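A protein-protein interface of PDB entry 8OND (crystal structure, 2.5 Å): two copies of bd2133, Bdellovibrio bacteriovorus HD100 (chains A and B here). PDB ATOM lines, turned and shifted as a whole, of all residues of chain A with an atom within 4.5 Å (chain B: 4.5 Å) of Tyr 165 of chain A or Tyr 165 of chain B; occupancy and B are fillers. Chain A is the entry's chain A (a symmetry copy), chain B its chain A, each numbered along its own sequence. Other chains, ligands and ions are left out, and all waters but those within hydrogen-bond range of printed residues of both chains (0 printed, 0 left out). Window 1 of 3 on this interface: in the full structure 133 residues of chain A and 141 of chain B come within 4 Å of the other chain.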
ATOM      1  N   MET A 156     -13.136 -32.522 -29.203  1.00  0.00           N
ATOM      2  CA  MET A 156     -11.895 -32.658 -28.460  1.00  0.00           C
ATOM      3  C   MET A 156     -12.152 -33.495 -27.219  1.00  0.00           C
ATOM      4  O   MET A 156     -13.215 -33.381 -26.606  1.00  0.00           O
ATOM      5  CB  MET A 156     -11.329 -31.315 -28.029  1.00  0.00           C
ATOM      6  CG  MET A 156      -9.837 -31.361 -27.850  1.00  0.00           C
ATOM      7  SD  MET A 156      -9.313 -30.135 -26.653  1.00  0.00           S
ATOM      8  CE  MET A 156      -7.876 -30.977 -25.995  1.00  0.00           C
ATOM      9  N   VAL A 157     -11.178 -34.313 -26.838  1.00  0.00           N
ATOM     10  CA  VAL A 157     -11.285 -35.111 -25.623  1.00  0.00           C
ATOM     11  C   VAL A 157      -9.948 -35.088 -24.899  1.00  0.00           C
ATOM     12  O   VAL A 157      -8.887 -35.059 -25.527  1.00  0.00           O
ATOM     13  CB  VAL A 157     -11.735 -36.560 -25.916  1.00  0.00           C
ATOM     14  CG1 VAL A 157     -10.661 -37.337 -26.667  1.00  0.00           C
ATOM     15  CG2 VAL A 157     -12.107 -37.272 -24.628  1.00  0.00           C
ATOM     16  N   ILE A 158     -10.004 -35.064 -23.575  1.00  0.00           N
ATOM     17  CA  ILE A 158      -8.835 -35.267 -22.736  1.00  0.00           C
ATOM     18  C   ILE A 158      -9.155 -36.398 -21.778  1.00  0.00           C
ATOM     19  O   ILE A 158     -10.291 -36.519 -21.309  1.00  0.00           O
ATOM     20  CB  ILE A 158      -8.428 -33.993 -21.964  1.00  0.00           C
ATOM     21  CG1 ILE A 158      -9.607 -33.403 -21.213  1.00  0.00           C
ATOM     22  CG2 ILE A 158      -7.950 -32.943 -22.923  1.00  0.00           C
ATOM     23  CD1 ILE A 158      -9.175 -32.389 -20.194  1.00  0.00           C
ATOM     24  N   ALA A 164      -8.346 -32.340 -16.733  1.00  0.00           N
ATOM     25  CA  ALA A 164      -9.003 -31.053 -16.558  1.00  0.00           C
ATOM     26  C   ALA A 164      -8.657 -30.103 -17.696  1.00  0.00           C
ATOM     27  O   ALA A 164      -7.518 -30.074 -18.168  1.00  0.00           O
ATOM     28  CB  ALA A 164      -8.616 -30.420 -15.218  1.00  0.00           C
ATOM     29  N   TYR A 165      -9.658 -29.339 -18.136  1.00  0.00           N
ATOM     30  CA  TYR A 165      -9.465 -28.195 -19.019  1.00  0.00           C
ATOM     31  C   TYR A 165      -9.227 -26.960 -18.154  1.00  0.00           C
ATOM     32  O   TYR A 165     -10.110 -26.561 -17.381  1.00  0.00           O
ATOM     33  CB  TYR A 165     -10.690 -27.962 -19.910  1.00  0.00           C
ATOM     34  CG  TYR A 165     -10.967 -28.990 -20.980  1.00  0.00           C
ATOM     35  CD1 TYR A 165     -10.291 -28.966 -22.189  1.00  0.00           C
ATOM     36  CD2 TYR A 165     -11.943 -29.963 -20.802  1.00  0.00           C
ATOM     37  CE1 TYR A 165     -10.563 -29.905 -23.185  1.00  0.00           C
ATOM     38  CE2 TYR A 165     -12.217 -30.902 -21.791  1.00  0.00           C
ATOM     39  CZ  TYR A 165     -11.530 -30.870 -22.979  1.00  0.00           C
ATOM     40  OH  TYR A 165     -11.804 -31.801 -23.965  1.00  0.00           O
ATOM     41  N   GLN A 166      -8.022 -26.402 -18.246  1.00  0.00           N
ATOM     42  CA  GLN A 166      -7.665 -25.290 -17.330  1.00  0.00           C
ATOM     43  C   GLN A 166      -7.628 -23.949 -18.062  1.00  0.00           C
ATOM     44  O   GLN A 166      -7.321 -23.937 -19.263  1.00  0.00           O
ATOM     45  CB  GLN A 166      -6.312 -25.596 -16.684  1.00  0.00           C
ATOM     46  CG  GLN A 166      -6.309 -26.867 -15.851  1.00  0.00           C
ATOM     47  CD  GLN A 166      -4.909 -27.286 -15.475  1.00  0.00           C
ATOM     48  OE1 GLN A 166      -3.927 -26.681 -15.894  1.00  0.00           O
ATOM     49  NE2 GLN A 166      -4.808 -28.342 -14.686  1.00  0.00           N
ATOM     50  N   LEU A 167      -7.930 -22.867 -17.344  1.00  0.00           N
ATOM     51  CA  LEU A 167      -7.865 -21.507 -17.932  1.00  0.00           C
ATOM     52  C   LEU A 167      -6.960 -20.653 -17.041  1.00  0.00           C
ATOM     53  O   LEU A 167      -7.365 -20.370 -15.902  1.00  0.00           O
ATOM     54  CB  LEU A 167      -9.280 -20.928 -17.988  1.00  0.00           C
ATOM     55  CG  LEU A 167     -10.282 -21.704 -18.841  1.00  0.00           C
ATOM     56  CD1 LEU A 167     -10.929 -22.819 -18.034  1.00  0.00           C
ATOM     57  CD2 LEU A 167     -11.346 -20.771 -19.396  1.00  0.00           C
ATOM     58  N   TRP A 177      -9.039 -20.887 -13.271  1.00  0.00           N
ATOM     59  CA  TRP A 177     -10.184 -21.792 -13.206  1.00  0.00           C
ATOM     60  C   TRP A 177      -9.889 -23.101 -13.921  1.00  0.00           C
ATOM     61  O   TRP A 177      -8.955 -23.201 -14.715  1.00  0.00           O
ATOM     62  CB  TRP A 177     -11.441 -21.169 -13.819  1.00  0.00           C
ATOM     63  CG  TRP A 177     -12.201 -20.339 -12.862  1.00  0.00           C
ATOM     64  CD1 TRP A 177     -12.169 -18.981 -12.743  1.00  0.00           C
ATOM     65  CD2 TRP A 177     -13.109 -20.809 -11.865  1.00  0.00           C
ATOM     66  NE1 TRP A 177     -13.006 -18.577 -11.736  1.00  0.00           N
ATOM     67  CE2 TRP A 177     -13.592 -19.685 -11.177  1.00  0.00           C
ATOM     68  CE3 TRP A 177     -13.556 -22.075 -11.486  1.00  0.00           C
ATOM     69  CZ2 TRP A 177     -14.504 -19.787 -10.135  1.00  0.00           C
ATOM     70  CZ3 TRP A 177     -14.459 -22.177 -10.447  1.00  0.00           C
ATOM     71  CH2 TRP A 177     -14.923 -21.040  -9.785  1.00  0.00           C
ATOM     72  N   GLN A 178     -10.708 -24.113 -13.640  1.00  0.00           N
ATOM     73  CA  GLN A 178     -10.628 -25.342 -14.418  1.00  0.00           C
ATOM     74  C   GLN A 178     -11.936 -26.115 -14.303  1.00  0.00           C
ATOM     75  O   GLN A 178     -12.656 -26.015 -13.302  1.00  0.00           O
ATOM     76  CB  GLN A 178      -9.444 -26.223 -13.990  1.00  0.00           C
ATOM     77  CG  GLN A 178      -9.698 -27.072 -12.764  1.00  0.00           C
ATOM     78  CD  GLN A 178      -8.482 -27.875 -12.353  1.00  0.00           C
ATOM     79  OE1 GLN A 178      -7.369 -27.592 -12.784  1.00  0.00           O
ATOM     80  NE2 GLN A 178      -8.692 -28.897 -11.528  1.00  0.00           N
ATOM     81  N   MET A 179     -12.229 -26.855 -15.380  1.00  0.00           N
ATOM     82  CA  MET A 179     -13.299 -27.849 -15.487  1.00  0.00           C
ATOM     83  C   MET A 179     -12.686 -29.241 -15.568  1.00  0.00           C
ATOM     84  O   MET A 179     -12.118 -29.611 -16.602  1.00  0.00           O
ATOM     85  CB  MET A 179     -14.154 -27.605 -16.730  1.00  0.00           C
ATOM     86  CG  MET A 179     -15.540 -28.215 -16.652  1.00  0.00           C
ATOM     87  SD  MET A 179     -16.501 -28.111 -18.190  1.00  0.00           S
ATOM     88  CE  MET A 179     -15.265 -28.317 -19.460  1.00  0.00           C
ATOM     89  N   MET B 156      -5.188 -30.056 -20.371  1.00  0.00           N
ATOM     90  CA  MET B 156      -5.048 -28.969 -21.326  1.00  0.00           C
ATOM     91  C   MET B 156      -5.183 -27.648 -20.593  1.00  0.00           C
ATOM     92  O   MET B 156      -5.983 -27.535 -19.662  1.00  0.00           O
ATOM     93  CB  MET B 156      -6.101 -29.024 -22.422  1.00  0.00           C
ATOM     94  CG  MET B 156      -5.632 -28.366 -23.690  1.00  0.00           C
ATOM     95  SD  MET B 156      -7.028 -27.744 -24.624  1.00  0.00           S
ATOM     96  CE  MET B 156      -6.236 -26.350 -25.422  1.00  0.00           C
ATOM     97  N   VAL B 157      -4.423 -26.647 -21.022  1.00  0.00           N
ATOM     98  CA  VAL B 157      -4.520 -25.313 -20.441  1.00  0.00           C
ATOM     99  C   VAL B 157      -4.456 -24.283 -21.556  1.00  0.00           C
ATOM    100  O   VAL B 157      -3.757 -24.472 -22.556  1.00  0.00           O
ATOM    101  CB  VAL B 157      -3.421 -25.059 -19.383  1.00  0.00           C
ATOM    102  CG1 VAL B 157      -2.039 -24.987 -20.021  1.00  0.00           C
ATOM    103  CG2 VAL B 157      -3.716 -23.791 -18.604  1.00  0.00           C
ATOM    104  N   ILE B 158      -5.217 -23.209 -21.401  1.00  0.00           N
ATOM    105  CA  ILE B 158      -5.104 -22.036 -22.252  1.00  0.00           C
ATOM    106  C   ILE B 158      -4.883 -20.839 -21.348  1.00  0.00           C
ATOM    107  O   ILE B 158      -5.453 -20.766 -20.255  1.00  0.00           O
ATOM    108  CB  ILE B 158      -6.346 -21.828 -23.144  1.00  0.00           C
ATOM    109  CG1 ILE B 158      -7.624 -21.851 -22.327  1.00  0.00           C
ATOM    110  CG2 ILE B 158      -6.449 -22.938 -24.149  1.00  0.00           C
ATOM    111  CD1 ILE B 158      -8.795 -21.313 -23.095  1.00  0.00           C
ATOM    112  N   ALA B 164     -10.426 -18.180 -23.536  1.00  0.00           N
ATOM    113  CA  ALA B 164     -11.731 -18.822 -23.556  1.00  0.00           C
ATOM    114  C   ALA B 164     -11.707 -20.081 -24.412  1.00  0.00           C
ATOM    115  O   ALA B 164     -11.066 -20.114 -25.465  1.00  0.00           O
ATOM    116  CB  ALA B 164     -12.805 -17.861 -24.076  1.00  0.00           C
ATOM    117  N   TYR B 165     -12.404 -21.117 -23.939  1.00  0.00           N
ATOM    118  CA  TYR B 165     -12.720 -22.299 -24.731  1.00  0.00           C
ATOM    119  C   TYR B 165     -14.044 -22.051 -25.449  1.00  0.00           C
ATOM    120  O   TYR B 165     -15.084 -21.873 -24.797  1.00  0.00           O
ATOM    121  CB  TYR B 165     -12.847 -23.545 -23.850  1.00  0.00           C
ATOM    122  CG  TYR B 165     -11.582 -24.070 -23.214  1.00  0.00           C
ATOM    123  CD1 TYR B 165     -10.700 -24.866 -23.925  1.00  0.00           C
ATOM    124  CD2 TYR B 165     -11.289 -23.807 -21.881  1.00  0.00           C
ATOM    125  CE1 TYR B 165      -9.541 -25.366 -23.330  1.00  0.00           C
ATOM    126  CE2 TYR B 165     -10.135 -24.302 -21.283  1.00  0.00           C
ATOM    127  CZ  TYR B 165      -9.267 -25.081 -22.007  1.00  0.00           C
ATOM    128  OH  TYR B 165      -8.120 -25.577 -21.412  1.00  0.00           O
ATOM    129  N   GLN B 166     -13.988 -21.980 -26.778  1.00  0.00           N
ATOM    130  CA  GLN B 166     -15.204 -21.596 -27.537  1.00  0.00           C
ATOM    131  C   GLN B 166     -15.808 -22.793 -28.272  1.00  0.00           C
ATOM    132  O   GLN B 166     -15.053 -23.698 -28.654  1.00  0.00           O
ATOM    133  CB  GLN B 166     -14.843 -20.479 -28.517  1.00  0.00           C
ATOM    134  CG  GLN B 166     -14.332 -19.217 -27.841  1.00  0.00           C
ATOM    135  CD  GLN B 166     -13.721 -18.259 -28.833  1.00  0.00           C
ATOM    136  OE1 GLN B 166     -13.600 -18.557 -30.018  1.00  0.00           O
ATOM    137  NE2 GLN B 166     -13.315 -17.098 -28.348  1.00  0.00           N
ATOM    138  N   LEU B 167     -17.128 -22.776 -28.458  1.00  0.00           N
ATOM    139  CA  LEU B 167     -17.816 -23.850 -29.215  1.00  0.00           C
ATOM    140  C   LEU B 167     -18.627 -23.192 -30.333  1.00  0.00           C
ATOM    141  O   LEU B 167     -19.608 -22.501 -30.011  1.00  0.00           O
ATOM    142  CB  LEU B 167     -18.728 -24.619 -28.256  1.00  0.00           C
ATOM    143  CG  LEU B 167     -18.031 -25.311 -27.087  1.00  0.00           C
ATOM    144  CD1 LEU B 167     -17.856 -24.354 -25.919  1.00  0.00           C
ATOM    145  CD2 LEU B 167     -18.815 -26.537 -26.649  1.00  0.00           C
ATOM    146  N   TRP B 177     -21.248 -20.628 -28.065  1.00  0.00           N
ATOM    147  CA  TRP B 177     -21.005 -20.545 -26.627  1.00  0.00           C
ATOM    148  C   TRP B 177     -19.516 -20.461 -26.326  1.00  0.00           C
ATOM    149  O   TRP B 177     -18.676 -20.772 -27.168  1.00  0.00           O
ATOM    150  CB  TRP B 177     -21.591 -21.746 -25.878  1.00  0.00           C
ATOM    151  CG  TRP B 177     -23.014 -21.566 -25.521  1.00  0.00           C
ATOM    152  CD1 TRP B 177     -24.097 -22.063 -26.185  1.00  0.00           C
ATOM    153  CD2 TRP B 177     -23.525 -20.823 -24.415  1.00  0.00           C
ATOM    154  NE1 TRP B 177     -25.252 -21.677 -25.554  1.00  0.00           N
ATOM    155  CE2 TRP B 177     -24.925 -20.910 -24.465  1.00  0.00           C
ATOM    156  CE3 TRP B 177     -22.931 -20.089 -23.387  1.00  0.00           C
ATOM    157  CZ2 TRP B 177     -25.741 -20.295 -23.525  1.00  0.00           C
ATOM    158  CZ3 TRP B 177     -23.743 -19.475 -22.456  1.00  0.00           C
ATOM    159  CH2 TRP B 177     -25.132 -19.582 -22.531  1.00  0.00           C
ATOM    160  N   GLN B 178     -19.195 -20.044 -25.103  1.00  0.00           N
ATOM    161  CA  GLN B 178     -17.810 -20.118 -24.659  1.00  0.00           C
ATOM    162  C   GLN B 178     -17.752 -20.106 -23.137  1.00  0.00           C
ATOM    163  O   GLN B 178     -18.631 -19.552 -22.464  1.00  0.00           O
ATOM    164  CB  GLN B 178     -16.953 -18.981 -25.238  1.00  0.00           C
ATOM    165  CG  GLN B 178     -17.069 -17.664 -24.502  1.00  0.00           C
ATOM    166  CD  GLN B 178     -16.251 -16.565 -25.147  1.00  0.00           C
ATOM    167  OE1 GLN B 178     -15.834 -16.687 -26.294  1.00  0.00           O
ATOM    168  NE2 GLN B 178     -16.001 -15.491 -24.404  1.00  0.00           N
ATOM    169  N   MET B 179     -16.707 -20.769 -22.624  1.00  0.00           N
ATOM    170  CA  MET B 179     -16.277 -20.765 -21.225  1.00  0.00           C
ATOM    171  C   MET B 179     -14.959 -20.012 -21.106  1.00  0.00           C
ATOM    172  O   MET B 179     -13.911 -20.523 -21.520  1.00  0.00           O
ATOM    173  CB  MET B 179     -16.088 -22.190 -20.703  1.00  0.00           C
ATOM    174  CG  MET B 179     -16.162 -22.306 -19.194  1.00  0.00           C
ATOM    175  SD  MET B 179     -15.744 -23.949 -18.539  1.00  0.00           S
ATOM    176  CE  MET B 179     -14.454 -24.510 -19.638  1.00  0.00           C
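Among the printed residues, merely in contact across the chains: Met 156 of chain A with Met 156 of chain B (3.6 Å), Tyr 165 of chain A with Met 156 of chain B (3.6 Å), Tyr 165 of chain A with Tyr 165 of chain B (3.7 Å), Gln 166 of chain A with Val 157 of chain B (3.3 Å), Leu 167 of chain A with Ile 158 of chain B (3.4 Å), Leu 167 of chain A with Tyr 165 of chain B (3.6 Å), Leu 167 of chain A with Met 179 of chain B (3.3 Å) and Met 179 of chain A with Met 179 of chain B (3.9 Å).
Hydrophobic or aromatic side chains of chain B within 4 Å of the printed part of chain A: Met 156, Val 157, Ile 158, Tyr 165 and Met 179. Of the 10 printed residues of chain A, 6 touch a printed residue of chain B. Hydrophobic or aromatic side chains of chain A within 4 Å of the printed part of chain B: Met 156, Tyr 165, Leu 167 and Met 179. Among the printed residues, no Asp or Glu carboxylate lies within 4 Å of a Lys or Arg side-chain nitrogen of the other chain.
Tyr 165 of chain B touches its own counterpart, Tyr 165 of chain A. Gln 166 of chain A touches Ile 158 of chain B, but with the chains exchanged Ile 158 of chain A does not touch Gln 166 of chain B (13.0 Å). Gln 166 of chain A touches Tyr 165 of chain B, but with the chains exchanged Tyr 165 of chain A does not touch Gln 166 of chain B (9.1 Å). Met 179 of chain A touches its own counterpart, Met 179 of chain B.
N of Met 156 of chain B lies within hydrogen-bond range of O of Ala 164 of chain A (3.2 Å). O of Met 156 of chain B lies within hydrogen-bond range of N of Gln 166 of chain A, 2.7 Å away. N of Ile 158 of chain B lies within hydrogen-bond range of O of Gln 166 of chain A (3.1 Å). The backbone carbonyl oxygen (O) of Gln 166 of chain A sits at hydrogen-bond distance from the side-chain hydroxyl (OH) of Tyr 165 of chain B (2.8 Å).
OH of Tyr 165 of chain B is in hydrogen-bond range of O of Met 156 of chain B (3.4 Å). The backbone carbonyl oxygen of Met 179 of chain B lies within hydrogen-bond range of the backbone NH of Tyr 165 of chain B (2.9 Å). The backbone carbonyl oxygen (O) of Met 156 of chain A is in hydrogen-bond range of the side-chain hydroxyl (OH) of Tyr 165 of chain A (3.4 Å). The backbone carbonyl oxygen (O) of Met 179 of chain A sits at hydrogen-bond distance from the backbone NH (N) of Tyr 165 of chain A. The side-chain amide nitrogen (NE2) of Gln 166 of chain A lies within hydrogen-bond range of the side-chain amide oxygen (OE1) of Gln 178 of chain A (3.3 Å). N of Leu 167 of chain A sits at hydrogen-bond distance from O of Trp 177 of chain A (2.8 Å).
Of chain B, only Met 156 (3.6 Å) and Tyr 165 (3.7 Å) come within 4 Å of Tyr 165 of chain A. Tyr 165 of chain B touches just these residues of chain A: Tyr 165, Gln 166 and Leu 167. Printed residues of chain B within 4 Å of Leu 167 of chain A: Ile 158 (3.4 Å), Tyr 165 (3.6 Å) and Met 179 (3.3 Å). Printed residues of chain B within 4 Å of Met 179 of chain A: Met 179. Of the printed residues of chain A, Met 179 of chain B touches Leu 167 and Met 179. The nearest printed residue of chain A that does not touch Tyr 165 of chain B is Ala 164 of chain A (5.6 Å). The nearest printed residue of chain B that does not touch Met 179 of chain A is Tyr 165 of chain B (6.5 Å).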
